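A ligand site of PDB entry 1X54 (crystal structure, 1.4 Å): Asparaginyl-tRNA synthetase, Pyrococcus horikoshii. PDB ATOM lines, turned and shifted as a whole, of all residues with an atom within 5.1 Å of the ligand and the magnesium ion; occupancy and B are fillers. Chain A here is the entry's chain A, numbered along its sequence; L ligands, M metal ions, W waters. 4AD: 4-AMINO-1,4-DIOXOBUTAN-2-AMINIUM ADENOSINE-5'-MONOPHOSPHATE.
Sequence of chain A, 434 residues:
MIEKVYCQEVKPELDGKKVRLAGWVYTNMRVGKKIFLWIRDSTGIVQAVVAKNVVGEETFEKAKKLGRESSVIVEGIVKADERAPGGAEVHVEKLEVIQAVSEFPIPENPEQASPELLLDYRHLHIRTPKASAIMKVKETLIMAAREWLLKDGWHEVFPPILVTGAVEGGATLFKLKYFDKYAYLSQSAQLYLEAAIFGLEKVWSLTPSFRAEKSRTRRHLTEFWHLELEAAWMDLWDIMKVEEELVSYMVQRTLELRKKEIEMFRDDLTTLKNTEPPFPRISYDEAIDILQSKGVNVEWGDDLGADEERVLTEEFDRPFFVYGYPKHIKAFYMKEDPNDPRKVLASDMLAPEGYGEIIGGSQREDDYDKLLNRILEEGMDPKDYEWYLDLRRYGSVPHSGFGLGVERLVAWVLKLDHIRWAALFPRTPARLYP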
ATOM      1  N   VAL A 167      -1.156   4.077   0.985  1.00  0.00           N
ATOM      2  CA  VAL A 167       0.282   3.980   0.774  1.00  0.00           C
ATOM      3  C   VAL A 167       0.934   5.252   1.268  1.00  0.00           C
ATOM      4  O   VAL A 167       2.047   5.222   1.804  1.00  0.00           O
ATOM      5  CB  VAL A 167       0.642   3.806  -0.739  1.00  0.00           C
ATOM      6  CG1 VAL A 167       2.133   3.532  -0.923  1.00  0.00           C
ATOM      7  CG2 VAL A 167      -0.163   2.703  -1.366  1.00  0.00           C
ATOM      8  N   GLU A 168       0.247   6.367   1.066  1.00  0.00           N
ATOM      9  CA  GLU A 168       0.816   7.679   1.346  1.00  0.00           C
ATOM     10  C   GLU A 168      -0.063   8.498   2.304  1.00  0.00           C
ATOM     11  O   GLU A 168      -0.178   9.725   2.162  1.00  0.00           O
ATOM     12  CB  GLU A 168       1.096   8.441   0.040  1.00  0.00           C
ATOM     13  CG  GLU A 168       2.033   7.694  -0.905  1.00  0.00           C
ATOM     14  CD  GLU A 168       3.452   7.524  -0.379  1.00  0.00           C
ATOM     15  OE1 GLU A 168       4.136   6.560  -0.825  1.00  0.00           O
ATOM     16  OE2 GLU A 168       3.912   8.335   0.462  1.00  0.00           O
ATOM     17  N   GLN A 187      -3.513   5.487  -4.258  1.00  0.00           N
ATOM     18  CA  GLN A 187      -2.602   6.636  -4.269  1.00  0.00           C
ATOM     19  C   GLN A 187      -1.283   6.333  -4.999  1.00  0.00           C
ATOM     20  O   GLN A 187      -0.510   7.238  -5.286  1.00  0.00           O
ATOM     21  CB  GLN A 187      -2.209   6.992  -2.836  1.00  0.00           C
ATOM     22  CG  GLN A 187      -3.352   7.474  -1.966  1.00  0.00           C
ATOM     23  CD  GLN A 187      -2.963   7.482  -0.506  1.00  0.00           C
ATOM     24  OE1 GLN A 187      -2.443   6.485   0.021  1.00  0.00           O
ATOM     25  NE2 GLN A 187      -3.159   8.617   0.162  1.00  0.00           N
ATOM     26  N   SER A 188      -1.023   5.046  -5.219  1.00  0.00           N
ATOM     27  CA  SER A 188       0.280   4.555  -5.666  1.00  0.00           C
ATOM     28  C   SER A 188       0.183   3.038  -5.761  1.00  0.00           C
ATOM     29  O   SER A 188      -0.423   2.394  -4.890  1.00  0.00           O
ATOM     30  CB  SER A 188       1.366   4.919  -4.654  1.00  0.00           C
ATOM     31  OG  SER A 188       2.530   4.151  -4.864  1.00  0.00           O
ATOM     32  N   GLN A 190       2.679   1.047  -5.458  1.00  0.00           N
ATOM     33  CA  GLN A 190       3.907   0.551  -4.873  1.00  0.00           C
ATOM     34  C   GLN A 190       3.762  -0.806  -4.158  1.00  0.00           C
ATOM     35  O   GLN A 190       4.582  -1.706  -4.359  1.00  0.00           O
ATOM     36  CB  GLN A 190       4.463   1.561  -3.878  1.00  0.00           C
ATOM     37  CG  GLN A 190       5.702   1.040  -3.171  1.00  0.00           C
ATOM     38  CD  GLN A 190       6.166   1.946  -2.070  1.00  0.00           C
ATOM     39  OE1 GLN A 190       6.100   3.168  -2.189  1.00  0.00           O
ATOM     40  NE2 GLN A 190       6.637   1.346  -0.987  1.00  0.00           N
ATOM     41  N   ARG A 211      -5.288  11.453  -5.370  1.00  0.00           N
ATOM     42  CA  ARG A 211      -4.937  12.121  -4.120  1.00  0.00           C
ATOM     43  C   ARG A 211      -6.001  13.134  -3.778  1.00  0.00           C
ATOM     44  O   ARG A 211      -6.213  14.091  -4.531  1.00  0.00           O
ATOM     45  CB  ARG A 211      -3.582  12.806  -4.238  1.00  0.00           C
ATOM     46  CG  ARG A 211      -2.407  11.899  -4.666  1.00  0.00           C
ATOM     47  CD  ARG A 211      -1.979  10.907  -3.602  1.00  0.00           C
ATOM     48  NE  ARG A 211      -0.887  10.067  -4.078  1.00  0.00           N
ATOM     49  CZ  ARG A 211       0.400  10.201  -3.756  1.00  0.00           C
ATOM     50  NH1 ARG A 211       1.301   9.384  -4.277  1.00  0.00           N
ATOM     51  NH2 ARG A 211       0.783  11.163  -2.902  1.00  0.00           N
ATOM     52  N   GLU A 213      -6.323  15.779  -2.287  1.00  0.00           N
ATOM     53  CA  GLU A 213      -5.531  16.881  -1.776  1.00  0.00           C
ATOM     54  C   GLU A 213      -6.380  18.131  -1.889  1.00  0.00           C
ATOM     55  O   GLU A 213      -6.727  18.549  -2.986  1.00  0.00           O
ATOM     56  CB  GLU A 213      -4.231  17.009  -2.592  1.00  0.00           C
ATOM     57  CG  GLU A 213      -3.330  18.188  -2.209  1.00  0.00           C
ATOM     58  CD  GLU A 213      -2.839  18.107  -0.765  1.00  0.00           C
ATOM     59  OE1 GLU A 213      -2.174  17.118  -0.412  1.00  0.00           O
ATOM     60  OE2 GLU A 213      -3.123  19.045   0.009  1.00  0.00           O
ATOM     61  N   ARG A 219       1.180  22.677  -8.265  1.00  0.00           N
ATOM     62  CA  ARG A 219       1.925  21.410  -8.406  1.00  0.00           C
ATOM     63  C   ARG A 219       1.112  20.164  -8.029  1.00  0.00           C
ATOM     64  O   ARG A 219       1.638  19.046  -8.027  1.00  0.00           O
ATOM     65  CB  ARG A 219       3.251  21.432  -7.599  1.00  0.00           C
ATOM     66  CG  ARG A 219       3.085  21.588  -6.084  1.00  0.00           C
ATOM     67  CD  ARG A 219       4.092  20.768  -5.235  1.00  0.00           C
ATOM     68  NE  ARG A 219       5.481  21.191  -5.426  1.00  0.00           N
ATOM     69  CZ  ARG A 219       6.542  20.661  -4.802  1.00  0.00           C
ATOM     70  NH1 ARG A 219       7.756  21.131  -5.057  1.00  0.00           N
ATOM     71  NH2 ARG A 219       6.400  19.669  -3.926  1.00  0.00           N
ATOM     72  N   HIS A 220      -0.159  20.340  -7.705  1.00  0.00           N
ATOM     73  CA  HIS A 220      -1.002  19.212  -7.286  1.00  0.00           C
ATOM     74  C   HIS A 220      -2.207  19.021  -8.187  1.00  0.00           C
ATOM     75  O   HIS A 220      -2.891  19.983  -8.538  1.00  0.00           O
ATOM     76  CB  HIS A 220      -1.478  19.406  -5.843  1.00  0.00           C
ATOM     77  CG  HIS A 220      -0.388  19.221  -4.832  1.00  0.00           C
ATOM     78  ND1 HIS A 220       0.280  20.286  -4.252  1.00  0.00           N
ATOM     79  CD2 HIS A 220       0.172  18.106  -4.306  1.00  0.00           C
ATOM     80  CE1 HIS A 220       1.187  19.838  -3.411  1.00  0.00           C
ATOM     81  NE2 HIS A 220       1.143  18.508  -3.426  1.00  0.00           N
ATOM     82  N   LEU A 221      -2.439  17.771  -8.569  1.00  0.00           N
ATOM     83  CA  LEU A 221      -3.681  17.348  -9.199  1.00  0.00           C
ATOM     84  C   LEU A 221      -4.332  16.356  -8.271  1.00  0.00           C
ATOM     85  O   LEU A 221      -3.654  15.830  -7.373  1.00  0.00           O
ATOM     86  CB  LEU A 221      -3.367  16.670 -10.540  1.00  0.00           C
ATOM     87  CG  LEU A 221      -2.748  17.569 -11.611  1.00  0.00           C
ATOM     88  CD1 LEU A 221      -2.253  16.723 -12.806  1.00  0.00           C
ATOM     89  CD2 LEU A 221      -3.736  18.666 -12.053  1.00  0.00           C
ATOM     90  N   PHE A 224      -3.411  11.879 -11.199  1.00  0.00           N
ATOM     91  CA  PHE A 224      -2.200  12.101 -12.001  1.00  0.00           C
ATOM     92  C   PHE A 224      -1.642  10.774 -12.488  1.00  0.00           C
ATOM     93  O   PHE A 224      -2.017   9.715 -11.961  1.00  0.00           O
ATOM     94  CB  PHE A 224      -1.143  12.900 -11.206  1.00  0.00           C
ATOM     95  CG  PHE A 224      -0.492  12.136 -10.097  1.00  0.00           C
ATOM     96  CD1 PHE A 224       0.743  11.484 -10.322  1.00  0.00           C
ATOM     97  CD2 PHE A 224      -1.056  12.092  -8.819  1.00  0.00           C
ATOM     98  CE1 PHE A 224       1.363  10.779  -9.290  1.00  0.00           C
ATOM     99  CE2 PHE A 224      -0.425  11.365  -7.785  1.00  0.00           C
ATOM    100  CZ  PHE A 224       0.784  10.726  -8.027  1.00  0.00           C
ATOM    101  N   HIS A 226       1.345   8.137 -12.889  1.00  0.00           N
ATOM    102  CA  HIS A 226       2.366   7.787 -11.924  1.00  0.00           C
ATOM    103  C   HIS A 226       3.172   6.617 -12.499  1.00  0.00           C
ATOM    104  O   HIS A 226       2.630   5.531 -12.690  1.00  0.00           O
ATOM    105  CB  HIS A 226       1.632   7.354 -10.651  1.00  0.00           C
ATOM    106  CG  HIS A 226       2.464   7.409  -9.414  1.00  0.00           C
ATOM    107  ND1 HIS A 226       1.922   7.146  -8.175  1.00  0.00           N
ATOM    108  CD2 HIS A 226       3.780   7.693  -9.203  1.00  0.00           C
ATOM    109  CE1 HIS A 226       2.868   7.270  -7.249  1.00  0.00           C
ATOM    110  NE2 HIS A 226       4.005   7.588  -7.843  1.00  0.00           N
ATOM    111  N   GLU A 228       5.950   4.007 -11.931  1.00  0.00           N
ATOM    112  CA  GLU A 228       6.545   3.447 -10.726  1.00  0.00           C
ATOM    113  C   GLU A 228       7.375   2.238 -11.059  1.00  0.00           C
ATOM    114  O   GLU A 228       6.967   1.416 -11.870  1.00  0.00           O
ATOM    115  CB  GLU A 228       5.450   3.096  -9.709  1.00  0.00           C
ATOM    116  CG  GLU A 228       4.624   4.320  -9.303  1.00  0.00           C
ATOM    117  CD  GLU A 228       3.546   4.006  -8.278  1.00  0.00           C
ATOM    118  OE1 GLU A 228       3.832   4.113  -7.070  1.00  0.00           O
ATOM    119  OE2 GLU A 228       2.411   3.670  -8.698  1.00  0.00           O
ATOM    120  N   LEU A 229       8.521   2.124 -10.393  1.00  0.00           N
ATOM    121  CA  LEU A 229       9.443   0.995 -10.559  1.00  0.00           C
ATOM    122  C   LEU A 229       9.713   0.375  -9.196  1.00  0.00           C
ATOM    123  O   LEU A 229       9.774   1.105  -8.181  1.00  0.00           O
ATOM    124  CB  LEU A 229      10.796   1.456 -11.139  1.00  0.00           C
ATOM    125  CG  LEU A 229      10.908   1.650 -12.653  1.00  0.00           C
ATOM    126  CD1 LEU A 229      10.036   2.783 -13.203  1.00  0.00           C
ATOM    127  CD2 LEU A 229      12.399   1.851 -13.019  1.00  0.00           C
ATOM    128  N   GLU A 230       9.919  -0.938  -9.171  1.00  0.00           N
ATOM    129  CA  GLU A 230      10.336  -1.613  -7.934  1.00  0.00           C
ATOM    130  C   GLU A 230      11.277  -2.744  -8.317  1.00  0.00           C
ATOM    131  O   GLU A 230      11.044  -3.412  -9.323  1.00  0.00           O
ATOM    132  CB  GLU A 230       9.098  -2.164  -7.195  1.00  0.00           C
ATOM    133  CG  GLU A 230       9.343  -2.585  -5.747  1.00  0.00           C
ATOM    134  CD  GLU A 230       9.378  -1.423  -4.781  1.00  0.00           C
ATOM    135  OE1 GLU A 230       8.758  -0.370  -5.059  1.00  0.00           O
ATOM    136  OE2 GLU A 230       9.999  -1.586  -3.712  1.00  0.00           O
ATOM    137  N   TYR A 333       6.635   2.641   5.304  1.00  0.00           N
ATOM    138  CA  TYR A 333       7.284   1.479   4.694  1.00  0.00           C
ATOM    139  C   TYR A 333       8.787   1.630   4.472  1.00  0.00           C
ATOM    140  O   TYR A 333       9.433   0.725   3.955  1.00  0.00           O
ATOM    141  CB  TYR A 333       6.605   1.176   3.343  1.00  0.00           C
ATOM    142  CG  TYR A 333       6.542   2.386   2.416  1.00  0.00           C
ATOM    143  CD1 TYR A 333       7.698   2.885   1.825  1.00  0.00           C
ATOM    144  CD2 TYR A 333       5.322   3.030   2.141  1.00  0.00           C
ATOM    145  CE1 TYR A 333       7.670   3.980   0.980  1.00  0.00           C
ATOM    146  CE2 TYR A 333       5.282   4.133   1.296  1.00  0.00           C
ATOM    147  CZ  TYR A 333       6.451   4.613   0.724  1.00  0.00           C
ATOM    148  OH  TYR A 333       6.439   5.717  -0.107  1.00  0.00           O
ATOM    149  N   ASP A 348      14.358  11.959  -2.649  1.00  0.00           N
ATOM    150  CA  ASP A 348      13.512  12.619  -3.642  1.00  0.00           C
ATOM    151  C   ASP A 348      14.394  13.213  -4.725  1.00  0.00           C
ATOM    152  O   ASP A 348      15.510  13.667  -4.444  1.00  0.00           O
ATOM    153  CB  ASP A 348      12.704  13.759  -3.002  1.00  0.00           C
ATOM    154  CG  ASP A 348      11.675  13.279  -2.000  1.00  0.00           C
ATOM    155  OD1 ASP A 348      11.270  12.097  -2.021  1.00  0.00           O
ATOM    156  OD2 ASP A 348      11.218  14.043  -1.128  1.00  0.00           O
ATOM    157  N   GLU A 357       9.998  18.582  -6.433  1.00  0.00           N
ATOM    158  CA  GLU A 357       9.950  17.111  -6.504  1.00  0.00           C
ATOM    159  C   GLU A 357       9.279  16.538  -7.761  1.00  0.00           C
ATOM    160  O   GLU A 357       8.107  16.811  -8.038  1.00  0.00           O
ATOM    161  CB  GLU A 357       9.265  16.550  -5.279  1.00  0.00           C
ATOM    162  CG  GLU A 357       9.269  15.022  -5.222  1.00  0.00           C
ATOM    163  CD  GLU A 357       8.670  14.486  -3.956  1.00  0.00           C
ATOM    164  OE1 GLU A 357       7.952  13.463  -4.024  1.00  0.00           O
ATOM    165  OE2 GLU A 357       8.919  15.087  -2.886  1.00  0.00           O
ATOM    166  N   ILE A 358      10.021  15.708  -8.493  1.00  0.00           N
ATOM    167  CA  ILE A 358       9.443  14.911  -9.580  1.00  0.00           C
ATOM    168  C   ILE A 358       9.420  13.411  -9.291  1.00  0.00           C
ATOM    169  O   ILE A 358       8.587  12.694  -9.870  1.00  0.00           O
ATOM    170  CB  ILE A 358      10.127  15.198 -10.911  1.00  0.00           C
ATOM    171  CG1 ILE A 358      11.630  14.956 -10.825  1.00  0.00           C
ATOM    172  CG2 ILE A 358       9.814  16.637 -11.379  1.00  0.00           C
ATOM    173  CD1 ILE A 358      12.282  14.919 -12.196  1.00  0.00           C
ATOM    174  N   ILE A 359      10.308  12.943  -8.407  1.00  0.00           N
ATOM    175  CA  ILE A 359      10.311  11.527  -7.978  1.00  0.00           C
ATOM    176  C   ILE A 359      10.419  11.444  -6.467  1.00  0.00           C
ATOM    177  O   ILE A 359      11.213  12.165  -5.841  1.00  0.00           O
ATOM    178  CB  ILE A 359      11.511  10.750  -8.579  1.00  0.00           C
ATOM    179  CG1 ILE A 359      11.361  10.631 -10.098  1.00  0.00           C
ATOM    180  CG2 ILE A 359      11.658   9.322  -7.921  1.00  0.00           C
ATOM    181  CD1 ILE A 359      12.523   9.942 -10.775  1.00  0.00           C
ATOM    182  N   GLY A 360       9.630  10.542  -5.886  1.00  0.00           N
ATOM    183  CA  GLY A 360       9.801  10.115  -4.486  1.00  0.00           C
ATOM    184  C   GLY A 360      10.093   8.626  -4.488  1.00  0.00           C
ATOM    185  O   GLY A 360       9.366   7.853  -5.103  1.00  0.00           O
ATOM    186  N   GLY A 361      11.172   8.224  -3.802  1.00  0.00           N
ATOM    187  CA  GLY A 361      11.499   6.795  -3.708  1.00  0.00           C
ATOM    188  C   GLY A 361      12.164   6.434  -2.393  1.00  0.00           C
ATOM    189  O   GLY A 361      12.499   7.313  -1.569  1.00  0.00           O
ATOM    190  N   SER A 362      12.375   5.145  -2.177  1.00  0.00           N
ATOM    191  CA  SER A 362      13.101   4.702  -0.998  1.00  0.00           C
ATOM    192  C   SER A 362      13.514   3.271  -1.108  1.00  0.00           C
ATOM    193  O   SER A 362      13.006   2.515  -1.940  1.00  0.00           O
ATOM    194  CB  SER A 362      12.256   4.876   0.282  1.00  0.00           C
ATOM    195  OG  SER A 362      11.408   3.761   0.514  1.00  0.00           O
ATOM    196  N   ARG A 364      12.963  -0.159   0.895  1.00  0.00           N
ATOM    197  CA  ARG A 364      11.801  -0.575   1.680  1.00  0.00           C
ATOM    198  C   ARG A 364      12.235  -1.375   2.908  1.00  0.00           C
ATOM    199  O   ARG A 364      13.237  -2.114   2.874  1.00  0.00           O
ATOM    200  CB  ARG A 364      10.870  -1.463   0.834  1.00  0.00           C
ATOM    201  CG  ARG A 364      10.615  -0.971  -0.584  1.00  0.00           C
ATOM    202  CD  ARG A 364      10.270   0.482  -0.704  1.00  0.00           C
ATOM    203  NE  ARG A 364       9.837   0.771  -2.066  1.00  0.00           N
ATOM    204  CZ  ARG A 364       9.474   1.971  -2.479  1.00  0.00           C
ATOM    205  NH1 ARG A 364       9.040   2.140  -3.722  1.00  0.00           N
ATOM    206  NH2 ARG A 364       9.573   3.032  -1.671  1.00  0.00           N
ATOM    207  N   GLY A 401      12.361   1.106  -4.612  1.00  0.00           N
ATOM    208  CA  GLY A 401      11.582   1.543  -5.757  1.00  0.00           C
ATOM    209  C   GLY A 401      11.282   3.041  -5.648  1.00  0.00           C
ATOM    210  O   GLY A 401      11.750   3.721  -4.736  1.00  0.00           O
ATOM    211  N   PHE A 402      10.500   3.541  -6.590  1.00  0.00           N
ATOM    212  CA  PHE A 402      10.199   4.957  -6.668  1.00  0.00           C
ATOM    213  C   PHE A 402       9.008   5.204  -7.579  1.00  0.00           C
ATOM    214  O   PHE A 402       8.618   4.345  -8.392  1.00  0.00           O
ATOM    215  CB  PHE A 402      11.386   5.765  -7.187  1.00  0.00           C
ATOM    216  CG  PHE A 402      11.759   5.506  -8.619  1.00  0.00           C
ATOM    217  CD1 PHE A 402      11.220   6.281  -9.642  1.00  0.00           C
ATOM    218  CD2 PHE A 402      12.682   4.498  -8.935  1.00  0.00           C
ATOM    219  CE1 PHE A 402      11.585   6.057 -10.973  1.00  0.00           C
ATOM    220  CE2 PHE A 402      13.074   4.276 -10.252  1.00  0.00           C
ATOM    221  CZ  PHE A 402      12.523   5.058 -11.274  1.00  0.00           C
ATOM    222  N   GLY A 403       8.461   6.412  -7.464  1.00  0.00           N
ATOM    223  CA  GLY A 403       7.376   6.864  -8.331  1.00  0.00           C
ATOM    224  C   GLY A 403       7.716   8.226  -8.900  1.00  0.00           C
ATOM    225  O   GLY A 403       8.146   9.124  -8.172  1.00  0.00           O
ATOM    226  N   LEU A 404       7.500   8.355 -10.212  1.00  0.00           N
ATOM    227  CA  LEU A 404       7.655   9.590 -10.958  1.00  0.00           C
ATOM    228  C   LEU A 404       6.275  10.166 -11.326  1.00  0.00           C
ATOM    229  O   LEU A 404       5.409   9.462 -11.854  1.00  0.00           O
ATOM    230  CB  LEU A 404       8.442   9.294 -12.253  1.00  0.00           C
ATOM    231  CG  LEU A 404       8.392  10.452 -13.255  1.00  0.00           C
ATOM    232  CD1 LEU A 404       9.283  11.629 -12.882  1.00  0.00           C
ATOM    233  CD2 LEU A 404       8.559  10.028 -14.700  1.00  0.00           C
ATOM    234  N   GLY A 405       6.074  11.462 -11.045  1.00  0.00           N
ATOM    235  CA  GLY A 405       4.874  12.166 -11.448  1.00  0.00           C
ATOM    236  C   GLY A 405       5.028  12.646 -12.888  1.00  0.00           C
ATOM    237  O   GLY A 405       5.848  13.543 -13.169  1.00  0.00           O
ATOM    238  N   ARG A 408       4.235  16.320 -13.360  1.00  0.00           N
ATOM    239  CA  ARG A 408       5.302  17.142 -12.768  1.00  0.00           C
ATOM    240  C   ARG A 408       6.494  17.230 -13.701  1.00  0.00           C
ATOM    241  O   ARG A 408       7.092  18.287 -13.859  1.00  0.00           O
ATOM    242  CB  ARG A 408       5.744  16.577 -11.413  1.00  0.00           C
ATOM    243  CG  ARG A 408       4.710  16.717 -10.311  1.00  0.00           C
ATOM    244  CD  ARG A 408       4.938  17.885  -9.335  1.00  0.00           C
ATOM    245  NE  ARG A 408       4.030  17.831  -8.197  1.00  0.00           N
ATOM    246  CZ  ARG A 408       4.319  17.410  -6.953  1.00  0.00           C
ATOM    247  NH1 ARG A 408       5.522  16.977  -6.603  1.00  0.00           N
ATOM    248  NH2 ARG A 408       3.354  17.445  -6.032  1.00  0.00           N
ATOM    249  N   ILE A 419       0.651  22.763 -13.227  1.00  0.00           N
ATOM    250  CA  ILE A 419       0.678  21.352 -13.589  1.00  0.00           C
ATOM    251  C   ILE A 419      -0.575  20.933 -14.379  1.00  0.00           C
ATOM    252  O   ILE A 419      -0.538  19.986 -15.190  1.00  0.00           O
ATOM    253  CB  ILE A 419       0.867  20.516 -12.314  1.00  0.00           C
ATOM    254  CG1 ILE A 419       1.263  19.095 -12.667  1.00  0.00           C
ATOM    255  CG2 ILE A 419      -0.365  20.597 -11.377  1.00  0.00           C
ATOM    256  CD1 ILE A 419       1.526  18.231 -11.441  1.00  0.00           C
HETATM  257  O2P 4AD L   1       6.218  11.091  -3.311  1.00  0.00           O
HETATM  258  P   4AD L   1       4.996  10.292  -3.615  1.00  0.00           P
HETATM  259  O1P 4AD L   1       3.743  10.499  -2.806  1.00  0.00           O
HETATM  260  O3P 4AD L   1       5.475   8.758  -3.466  1.00  0.00           O
HETATM  261  C   4AD L   1       4.685   7.584  -3.689  1.00  0.00           C
HETATM  262  O   4AD L   1       3.472   7.630  -3.921  1.00  0.00           O
HETATM  263  CA  4AD L   1       5.468   6.325  -3.600  1.00  0.00           C
HETATM  264  N   4AD L   1       4.608   5.235  -3.179  1.00  0.00           N
HETATM  265  CB  4AD L   1       6.021   6.118  -5.017  1.00  0.00           C
HETATM  266  CG  4AD L   1       6.844   4.849  -5.075  1.00  0.00           C
HETATM  267  OD1 4AD L   1       7.842   4.729  -4.372  1.00  0.00           O
HETATM  268  ND2 4AD L   1       6.418   3.913  -5.921  1.00  0.00           N
HETATM  269  O5' 4AD L   1       4.567  10.405  -5.164  1.00  0.00           O
HETATM  270  C5' 4AD L   1       5.514  10.082  -6.193  1.00  0.00           C
HETATM  271  C4' 4AD L   1       5.486  11.233  -7.186  1.00  0.00           C
HETATM  272  C3' 4AD L   1       5.894  12.599  -6.617  1.00  0.00           C
HETATM  273  O3' 4AD L   1       7.311  12.751  -6.635  1.00  0.00           O
HETATM  274  C2' 4AD L   1       5.220  13.562  -7.565  1.00  0.00           C
HETATM  275  O2' 4AD L   1       6.028  13.660  -8.761  1.00  0.00           O
HETATM  276  C1' 4AD L   1       3.947  12.830  -7.940  1.00  0.00           C
HETATM  277  O4' 4AD L   1       4.152  11.452  -7.664  1.00  0.00           O
HETATM  278  N9  4AD L   1       2.747  13.348  -7.230  1.00  0.00           N
HETATM  279  C4  4AD L   1       1.812  14.157  -7.690  1.00  0.00           C
HETATM  280  N3  4AD L   1       1.652  14.730  -8.895  1.00  0.00           N
HETATM  281  C2  4AD L   1       0.578  15.512  -9.095  1.00  0.00           C
HETATM  282  N1  4AD L   1      -0.320  15.707  -8.114  1.00  0.00           N
HETATM  283  C6  4AD L   1      -0.197  15.165  -6.868  1.00  0.00           C
HETATM  284  N6  4AD L   1      -1.144  15.404  -5.935  1.00  0.00           N
HETATM  285  C5  4AD L   1       0.902  14.342  -6.616  1.00  0.00           C
HETATM  286  N7  4AD L   1       1.314  13.641  -5.510  1.00  0.00           N
HETATM  287  C8  4AD L   1       2.563  12.952  -5.844  1.00  0.00           C
HETATM  288 MG    MG M   1       6.925  12.711  -2.226  1.00  0.00          MG
HETATM  289  O   HOH W   1       7.417   1.352  -6.643  1.00  0.00           O
HETATM  290  O   HOH W   2       8.577   5.907  -2.003  1.00  0.00           O
HETATM  291  O   HOH W   3       5.157  13.828  -2.981  1.00  0.00           O
HETATM  292  O   HOH W   4       7.790  14.415  -0.861  1.00  0.00           O
HETATM  293  O   HOH W   5       3.332  10.961  -0.062  1.00  0.00           O
HETATM  294  O   HOH W   6       8.611  11.615  -1.562  1.00  0.00           O
HETATM  295  O   HOH W   7       2.561  14.317 -11.805  1.00  0.00           O
HETATM  296  O   HOH W   8       5.898  11.971  -0.400  1.00  0.00           O
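The backbone carbonyl oxygen of Phe 402 sits close to a nitrogen (ND2) of the ligand (3.3 Å).
OE1 of Glu 228 is in hydrogen-bond range of ND2 of the ligand (2.8 Å).
An oxygen (O3') of the ligand is in hydrogen-bond range of the backbone NH (N) of Gly 360 (3.3 Å).
The side-chain hydroxyl (OG) of Ser 188 sits at hydrogen-bond distance from a nitrogen (N) of the ligand (2.9 Å).
OE1 of Glu 168 is in salt-bridge range of N of the ligand (2.7 Å).
An oxygen (O2') of the ligand is in hydrogen-bond range of the backbone NH of Gly 405.
NH1 of Arg 364 is in hydrogen-bond range of OD1 of the ligand (2.9 Å).
The backbone NH (N) of Leu 221 lies within hydrogen-bond range of a nitrogen (N1) of the ligand, at 3.0 Å.
The backbone NH of Ile 359 sits close to an oxygen (O3') of the ligand.
The side-chain amide oxygen (OE1) of Gln 190 is in hydrogen-bond range of a nitrogen (N) of the ligand, at 2.7 Å.
A nitrogen (N6) of the ligand is in hydrogen-bond range of the backbone carbonyl oxygen (O) of Leu 221, at 2.9 Å.
An oxygen (O2') of the ligand is in hydrogen-bond range of the backbone carbonyl oxygen (O) of Ile 358.
The guanidinium group of Arg 211 lies within salt-bridge range of an oxygen (O1P) of the ligand, at 3.0 Å.
The backbone carbonyl oxygen (O) of Glu 357 sits at hydrogen-bond distance from the guanidinium group (NH1) of Arg 408, at 3.0 Å.
The backbone NH (N) of Gln 190 is in hydrogen-bond range of the side-chain hydroxyl (OG) of Ser 188, at 3.2 Å.
The backbone carbonyl oxygen (O) of Ile 358 is in hydrogen-bond range of the backbone NH (N) of Gly 405.
The backbone NH of Gly 403 lies within hydrogen-bond range of the backbone carbonyl oxygen of Gly 360.
OG of Ser 188 sits at hydrogen-bond distance from OE1 of Glu 228.
The guanidinium group (NE) of Arg 364 sits close to the side-chain amide nitrogen (NE2) of Gln 190, 3.4 Å away.
The guanidinium group (NE) of Arg 408 sits at hydrogen-bond distance from the backbone carbonyl oxygen (O) of Arg 219 (2.7 Å).
The side-chain hydroxyl of Tyr 333 lies within hydrogen-bond range of the side-chain carboxylate of Glu 168 (2.6 Å).
Merely in contact with the ligand: Val 167 (3.8 Å), Arg 219 (3.8 Å), His 220 (3.4 Å), Phe 224 (3.3 Å), His 226 (3.3 Å), Tyr 333 (3.6 Å), Gly 403 (3.3 Å), Arg 408 (3.6 Å) and Ile 419 (3.7 Å).
Hydrophobic or aromatic side chains within 4 Å of the ligand: Val 167, His 220, Phe 224, His 226 and Ile 419.
22 residues have an atom within 4 Å of the ligand: Val 167, Glu 168, Ser 188, Gln 190, Arg 211, Arg 219, His 220, Leu 221, Phe 224, His 226, Glu 228, Tyr 333, Glu 357, Ile 358, Ile 359, Gly 360, Arg 364, Phe 402, Gly 403, Gly 405, Arg 408 and Ile 419.
The nearest printed residue that does not touch the ligand is Gly 401 (4.04 Å).
Of the 31 residues printed, 1 comes within 4 Å of the magnesium ion.
The nearest printed residue that does not touch the magnesium ion is Asp 348 (4.4 Å).
An oxygen (O2P) of the ligand is bound to the magnesium ion (2.1 Å).
The magnesium ion is bound by water W6 (2.1 Å).
The magnesium ion is bound by the side-chain carboxylate (OE1) of Glu 357, at 2.2 Å.
Water W8 binds the magnesium ion, 2.2 Å away.
Water W3 is bound to the magnesium ion, at 2.2 Å.
Water W4 binds the magnesium ion, 2.3 Å away.
Water W4 bridges the side-chain carboxylate of Glu 357 (2.4 Å) and the side-chain carboxylate of Asp 348 (3.5 Å).
Water W2 lies within hydrogen-bond range of OD1 of the ligand (2.7 Å), OH of Tyr 333 (2.9 Å) and NH2 of Arg 364 (3.1 Å).
Water W5 lies within hydrogen-bond range of OE2 of Glu 168 (2.7 Å) and O1P of the ligand (2.8 Å).
Water W1 lies within hydrogen-bond range of OE1 of Glu 230 (2.7 Å), O of Leu 229 (2.8 Å), ND2 of the ligand (2.8 Å) and NH1 of Arg 364 (3.4 Å).
Water W7 bridges the backbone NH of Arg 408 (3.0 Å) and a nitrogen (N3) of the ligand (3.1 Å).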
